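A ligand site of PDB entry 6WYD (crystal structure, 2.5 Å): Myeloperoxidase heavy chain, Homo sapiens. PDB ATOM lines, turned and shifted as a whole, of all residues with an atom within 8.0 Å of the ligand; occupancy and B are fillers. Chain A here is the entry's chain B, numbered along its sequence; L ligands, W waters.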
ATOM      1  N   ASN A  74      20.023  20.609  17.879  1.00  0.00           N
ATOM      2  CA  ASN A  74      21.073  21.548  18.295  1.00  0.00           C
ATOM      3  C   ASN A  74      21.674  21.265  19.674  1.00  0.00           C
ATOM      4  O   ASN A  74      22.833  21.620  19.926  1.00  0.00           O
ATOM      5  CB  ASN A  74      20.536  22.988  18.262  1.00  0.00           C
ATOM      6  CG  ASN A  74      20.297  23.572  16.895  1.00  0.00           C
ATOM      7  OD1 ASN A  74      20.758  23.075  15.859  1.00  0.00           O
ATOM      8  ND2 ASN A  74      19.591  24.708  16.870  1.00  0.00           N
ATOM      9  N   LEU A  75      20.876  20.665  20.598  1.00  0.00           N
ATOM     10  CA  LEU A  75      21.343  20.330  21.945  1.00  0.00           C
ATOM     11  C   LEU A  75      22.257  19.100  21.928  1.00  0.00           C
ATOM     12  O   LEU A  75      22.874  18.779  22.953  1.00  0.00           O
ATOM     13  CB  LEU A  75      20.166  20.086  22.899  1.00  0.00           C
ATOM     14  CG  LEU A  75      19.316  21.271  23.335  1.00  0.00           C
ATOM     15  CD1 LEU A  75      18.056  20.786  23.998  1.00  0.00           C
ATOM     16  CD2 LEU A  75      20.079  22.190  24.251  1.00  0.00           C
ATOM     17  N   ARG A  76      22.327  18.412  20.771  1.00  0.00           N
ATOM     18  CA  ARG A  76      23.116  17.193  20.582  1.00  0.00           C
ATOM     19  C   ARG A  76      24.492  17.432  19.997  1.00  0.00           C
ATOM     20  O   ARG A  76      24.688  18.352  19.194  1.00  0.00           O
ATOM     21  CB  ARG A  76      22.386  16.199  19.686  1.00  0.00           C
ATOM     22  CG  ARG A  76      21.186  15.554  20.364  1.00  0.00           C
ATOM     23  CD  ARG A  76      20.398  14.749  19.377  1.00  0.00           C
ATOM     24  NE  ARG A  76      21.103  13.530  19.000  1.00  0.00           N
ATOM     25  CZ  ARG A  76      20.767  12.758  17.971  1.00  0.00           C
ATOM     26  NH1 ARG A  76      19.725  13.084  17.203  1.00  0.00           N
ATOM     27  NH2 ARG A  76      21.455  11.663  17.700  1.00  0.00           N
ATOM     28  N   ASN A  77      25.426  16.562  20.400  1.00  0.00           N
ATOM     29  CA  ASN A  77      26.802  16.545  19.934  1.00  0.00           C
ATOM     30  C   ASN A  77      26.833  15.714  18.633  1.00  0.00           C
ATOM     31  O   ASN A  77      26.821  14.481  18.665  1.00  0.00           O
ATOM     32  CB  ASN A  77      27.737  15.989  21.010  1.00  0.00           C
ATOM     33  CG  ASN A  77      29.162  15.879  20.559  1.00  0.00           C
ATOM     34  OD1 ASN A  77      29.659  16.657  19.735  1.00  0.00           O
ATOM     35  ND2 ASN A  77      29.840  14.860  21.045  1.00  0.00           N
ATOM     36  N   MET A  78      26.822  16.446  17.502  1.00  0.00           N
ATOM     37  CA  MET A  78      26.782  15.949  16.112  1.00  0.00           C
ATOM     38  C   MET A  78      28.176  15.761  15.479  1.00  0.00           C
ATOM     39  O   MET A  78      28.270  15.504  14.285  1.00  0.00           O
ATOM     40  CB  MET A  78      25.926  16.900  15.248  1.00  0.00           C
ATOM     41  CG  MET A  78      24.478  17.019  15.680  1.00  0.00           C
ATOM     42  SD  MET A  78      23.510  15.526  15.319  1.00  0.00           S
ATOM     43  CE  MET A  78      22.487  16.153  13.940  1.00  0.00           C
ATOM     44  N   SER A  79      29.248  15.881  16.289  1.00  0.00           N
ATOM     45  CA  SER A  79      30.652  15.757  15.881  1.00  0.00           C
ATOM     46  C   SER A  79      31.116  14.296  15.811  1.00  0.00           C
ATOM     47  O   SER A  79      32.234  14.052  15.341  1.00  0.00           O
ATOM     48  CB  SER A  79      31.545  16.480  16.892  1.00  0.00           C
ATOM     49  OG  SER A  79      31.157  17.827  17.128  1.00  0.00           O
ATOM     50  N   ASN A  80      30.305  13.339  16.336  1.00  0.00           N
ATOM     51  CA  ASN A  80      30.652  11.910  16.463  1.00  0.00           C
ATOM     52  C   ASN A  80      29.425  10.973  16.656  1.00  0.00           C
ATOM     53  O   ASN A  80      28.281  11.407  16.589  1.00  0.00           O
ATOM     54  CB  ASN A  80      31.613  11.738  17.654  1.00  0.00           C
ATOM     55  CG  ASN A  80      31.180  12.504  18.875  1.00  0.00           C
ATOM     56  OD1 ASN A  80      30.143  12.232  19.480  1.00  0.00           O
ATOM     57  ND2 ASN A  80      31.952  13.532  19.222  1.00  0.00           N
ATOM     58  N   LEU A  82      28.806   9.123  19.424  1.00  0.00           N
ATOM     59  CA  LEU A  82      28.755   8.840  20.854  1.00  0.00           C
ATOM     60  C   LEU A  82      27.384   9.123  21.505  1.00  0.00           C
ATOM     61  O   LEU A  82      27.160   8.703  22.647  1.00  0.00           O
ATOM     62  CB  LEU A  82      29.897   9.577  21.584  1.00  0.00           C
ATOM     63  CG  LEU A  82      31.346   9.249  21.205  1.00  0.00           C
ATOM     64  CD1 LEU A  82      32.278   9.842  22.232  1.00  0.00           C
ATOM     65  CD2 LEU A  82      31.591   7.732  21.114  1.00  0.00           C
ATOM     66  N   LEU A  84      25.967  12.001  22.521  1.00  0.00           N
ATOM     67  CA  LEU A  84      26.156  12.892  23.642  1.00  0.00           C
ATOM     68  C   LEU A  84      25.384  14.168  23.446  1.00  0.00           C
ATOM     69  O   LEU A  84      24.997  14.495  22.324  1.00  0.00           O
ATOM     70  CB  LEU A  84      27.662  13.253  23.753  1.00  0.00           C
ATOM     71  CG  LEU A  84      28.663  12.128  23.984  1.00  0.00           C
ATOM     72  CD1 LEU A  84      30.104  12.640  23.776  1.00  0.00           C
ATOM     73  CD2 LEU A  84      28.480  11.477  25.357  1.00  0.00           C
ATOM     74  N   LEU A  85      25.175  14.912  24.536  1.00  0.00           N
ATOM     75  CA  LEU A  85      24.524  16.218  24.457  1.00  0.00           C
ATOM     76  C   LEU A  85      25.651  17.247  24.392  1.00  0.00           C
ATOM     77  O   LEU A  85      26.683  17.046  25.050  1.00  0.00           O
ATOM     78  CB  LEU A  85      23.589  16.486  25.669  1.00  0.00           C
ATOM     79  CG  LEU A  85      22.242  15.763  25.671  1.00  0.00           C
ATOM     80  CD1 LEU A  85      21.634  15.774  27.044  1.00  0.00           C
ATOM     81  CD2 LEU A  85      21.259  16.347  24.661  1.00  0.00           C
ATOM     82  N   ALA A  86      25.468  18.296  23.574  1.00  0.00           N
ATOM     83  CA  ALA A  86      26.434  19.381  23.418  1.00  0.00           C
ATOM     84  C   ALA A  86      26.746  20.037  24.770  1.00  0.00           C
ATOM     85  O   ALA A  86      25.844  20.284  25.576  1.00  0.00           O
ATOM     86  CB  ALA A  86      25.925  20.421  22.427  1.00  0.00           C
ATOM     87  N   VAL A  87      28.042  20.221  25.049  1.00  0.00           N
ATOM     88  CA  VAL A  87      28.552  20.794  26.294  1.00  0.00           C
ATOM     89  C   VAL A  87      29.269  22.101  25.950  1.00  0.00           C
ATOM     90  O   VAL A  87      29.690  22.287  24.794  1.00  0.00           O
ATOM     91  CB  VAL A  87      29.441  19.793  27.089  1.00  0.00           C
ATOM     92  CG1 VAL A  87      28.660  18.537  27.431  1.00  0.00           C
ATOM     93  CG2 VAL A  87      30.721  19.433  26.330  1.00  0.00           C
ATOM     94  N   ASN A  88      29.381  23.019  26.942  1.00  0.00           N
ATOM     95  CA  ASN A  88      30.060  24.300  26.748  1.00  0.00           C
ATOM     96  C   ASN A  88      31.480  24.047  26.308  1.00  0.00           C
ATOM     97  O   ASN A  88      32.175  23.214  26.896  1.00  0.00           O
ATOM     98  CB  ASN A  88      30.036  25.155  28.005  1.00  0.00           C
ATOM     99  CG  ASN A  88      30.322  26.605  27.697  1.00  0.00           C
ATOM    100  OD1 ASN A  88      31.455  27.001  27.457  1.00  0.00           O
ATOM    101  ND2 ASN A  88      29.300  27.420  27.598  1.00  0.00           N
ATOM    102  N   GLN A  89      31.878  24.712  25.227  1.00  0.00           N
ATOM    103  CA  GLN A  89      33.217  24.574  24.663  1.00  0.00           C
ATOM    104  C   GLN A  89      34.212  25.596  25.276  1.00  0.00           C
ATOM    105  O   GLN A  89      35.399  25.285  25.375  1.00  0.00           O
ATOM    106  CB  GLN A  89      33.173  24.680  23.119  1.00  0.00           C
ATOM    107  CG  GLN A  89      32.390  23.553  22.443  1.00  0.00           C
ATOM    108  CD  GLN A  89      33.078  22.220  22.537  1.00  0.00           C
ATOM    109  OE1 GLN A  89      34.041  21.935  21.814  1.00  0.00           O
ATOM    110  NE2 GLN A  89      32.571  21.352  23.400  1.00  0.00           N
ATOM    111  N   GLN A  92      34.420  24.852  31.672  1.00  0.00           N
ATOM    112  CA  GLN A  92      34.216  23.583  32.405  1.00  0.00           C
ATOM    113  C   GLN A  92      34.106  23.891  33.909  1.00  0.00           C
ATOM    114  O   GLN A  92      34.439  25.005  34.333  1.00  0.00           O
ATOM    115  CB  GLN A  92      35.361  22.596  32.187  1.00  0.00           C
ATOM    116  CG  GLN A  92      35.413  21.986  30.815  1.00  0.00           C
ATOM    117  CD  GLN A  92      36.616  21.078  30.737  1.00  0.00           C
ATOM    118  OE1 GLN A  92      37.768  21.542  30.693  1.00  0.00           O
ATOM    119  NE2 GLN A  92      36.368  19.773  30.776  1.00  0.00           N
ATOM    120  N   ALA A  97      31.461  18.967  32.665  1.00  0.00           N
ATOM    121  CA  ALA A  97      30.652  19.753  31.734  1.00  0.00           C
ATOM    122  C   ALA A  97      29.750  20.799  32.337  1.00  0.00           C
ATOM    123  O   ALA A  97      29.249  20.653  33.446  1.00  0.00           O
ATOM    124  CB  ALA A  97      29.852  18.831  30.838  1.00  0.00           C
ATOM    125  N   LEU A  98      29.550  21.874  31.554  1.00  0.00           N
ATOM    126  CA  LEU A  98      28.600  22.943  31.782  1.00  0.00           C
ATOM    127  C   LEU A  98      27.689  22.966  30.515  1.00  0.00           C
ATOM    128  O   LEU A  98      28.102  22.459  29.466  1.00  0.00           O
ATOM    129  CB  LEU A  98      29.303  24.302  31.961  1.00  0.00           C
ATOM    130  CG  LEU A  98      29.951  24.586  33.327  1.00  0.00           C
ATOM    131  CD1 LEU A  98      30.677  25.909  33.300  1.00  0.00           C
ATOM    132  CD2 LEU A  98      28.917  24.575  34.468  1.00  0.00           C
ATOM    133  N   PRO A 100      25.902  24.388  27.101  1.00  0.00           N
ATOM    134  CA  PRO A 100      26.474  25.347  26.142  1.00  0.00           C
ATOM    135  C   PRO A 100      25.710  26.663  26.174  1.00  0.00           C
ATOM    136  O   PRO A 100      24.601  26.700  26.716  1.00  0.00           O
ATOM    137  CB  PRO A 100      26.353  24.612  24.802  1.00  0.00           C
ATOM    138  CG  PRO A 100      25.288  23.585  24.982  1.00  0.00           C
ATOM    139  CD  PRO A 100      25.031  23.387  26.449  1.00  0.00           C
ATOM    140  N   LEU A 142      22.391  17.088  32.244  1.00  0.00           N
ATOM    141  CA  LEU A 142      23.181  17.082  31.003  1.00  0.00           C
ATOM    142  C   LEU A 142      24.372  16.088  31.194  1.00  0.00           C
ATOM    143  O   LEU A 142      24.687  15.347  30.268  1.00  0.00           O
ATOM    144  CB  LEU A 142      23.699  18.505  30.682  1.00  0.00           C
ATOM    145  CG  LEU A 142      24.731  18.646  29.529  1.00  0.00           C
ATOM    146  CD1 LEU A 142      24.071  19.014  28.237  1.00  0.00           C
ATOM    147  CD2 LEU A 142      25.786  19.680  29.873  1.00  0.00           C
ATOM    148  N   ASN A 146      25.253  11.965  29.298  1.00  0.00           N
ATOM    149  CA  ASN A 146      26.586  11.735  28.733  1.00  0.00           C
ATOM    150  C   ASN A 146      27.292  10.589  29.444  1.00  0.00           C
ATOM    151  O   ASN A 146      27.927   9.769  28.793  1.00  0.00           O
ATOM    152  CB  ASN A 146      27.383  13.041  28.643  1.00  0.00           C
ATOM    153  CG  ASN A 146      26.812  14.021  27.648  1.00  0.00           C
ATOM    154  OD1 ASN A 146      25.849  13.726  26.930  1.00  0.00           O
ATOM    155  ND2 ASN A 146      27.366  15.225  27.555  1.00  0.00           N
ATOM    156  N   THR A 150      28.084   6.874  27.705  1.00  0.00           N
ATOM    157  CA  THR A 150      29.477   6.426  27.780  1.00  0.00           C
ATOM    158  C   THR A 150      29.485   4.969  28.285  1.00  0.00           C
ATOM    159  O   THR A 150      30.162   4.126  27.686  1.00  0.00           O
ATOM    160  CB  THR A 150      30.332   7.438  28.560  1.00  0.00           C
ATOM    161  OG1 THR A 150      30.319   8.673  27.828  1.00  0.00           O
ATOM    162  CG2 THR A 150      31.765   6.979  28.769  1.00  0.00           C
HETATM  163  C1  LIG L   1      32.249  16.433  21.134  1.00  0.00           C
HETATM  164  C2  LIG L   1      32.247  17.722  21.940  1.00  0.00           C
HETATM  165  C3  LIG L   1      33.719  17.979  22.412  1.00  0.00           C
HETATM  166  C4  LIG L   1      34.474  16.698  22.980  1.00  0.00           C
HETATM  167  C5  LIG L   1      33.916  15.334  22.322  1.00  0.00           C
HETATM  168  C6  LIG L   1      34.211  13.927  22.893  1.00  0.00           C
HETATM  169  C7  LIG L   1      30.358  19.368  21.845  1.00  0.00           C
HETATM  170  C8  LIG L   1      29.760  20.474  21.038  1.00  0.00           C
HETATM  171  N1  LIG L   1      31.501  18.815  21.279  1.00  0.00           N
HETATM  172  O1  LIG L   1      33.686  18.958  23.456  1.00  0.00           O
HETATM  173  O2  LIG L   1      35.955  16.953  23.031  1.00  0.00           O
HETATM  174  O3  LIG L   1      32.458  15.384  22.087  1.00  0.00           O
HETATM  175  O4  LIG L   1      33.703  13.748  24.192  1.00  0.00           O
HETATM  176  O5  LIG L   1      29.873  19.010  22.909  1.00  0.00           O
HETATM  177  O   HOH W   1      29.237  16.586  24.073  1.00  0.00           O
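N of Val 87 lies within hydrogen-bond range of O5 of the ligand (3.1 Å). The side-chain amide nitrogen of Asn 80 sits at hydrogen-bond distance from an oxygen (O3) of the ligand (3.4 Å). NE2 of Gln 89 sits at hydrogen-bond distance from O1 of the ligand. An oxygen (O3) of the ligand is in hydrogen-bond range of the side-chain amide nitrogen (ND2) of Asn 77 (2.9 Å).
ND2 of Asn 77 sits at hydrogen-bond distance from OD1 of Asn 80. NE2 of Gln 89 lies within hydrogen-bond range of O of Val 87 (3.3 Å). N of Ala 86 is in hydrogen-bond range of O of Leu 75 (2.7 Å). N of Asn 77 lies within hydrogen-bond range of O of Leu 84, 2.9 Å away. OD1 of Asn 80 is in hydrogen-bond range of N of Leu 82, 3.4 Å away. OD1 of Asn 77 is in hydrogen-bond range of OG of Ser 79, at 3.2 Å.
Merely in contact with the ligand: Leu 84 and Ala 86. Of the 21 residues printed, 6 come within 4 Å of the ligand. The nearest printed residue that does not touch the ligand is Ser 79 (4.3 Å).
Water W1 bridges an oxygen (O5) of the ligand and the backbone carbonyl oxygen (O) of Leu 85.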
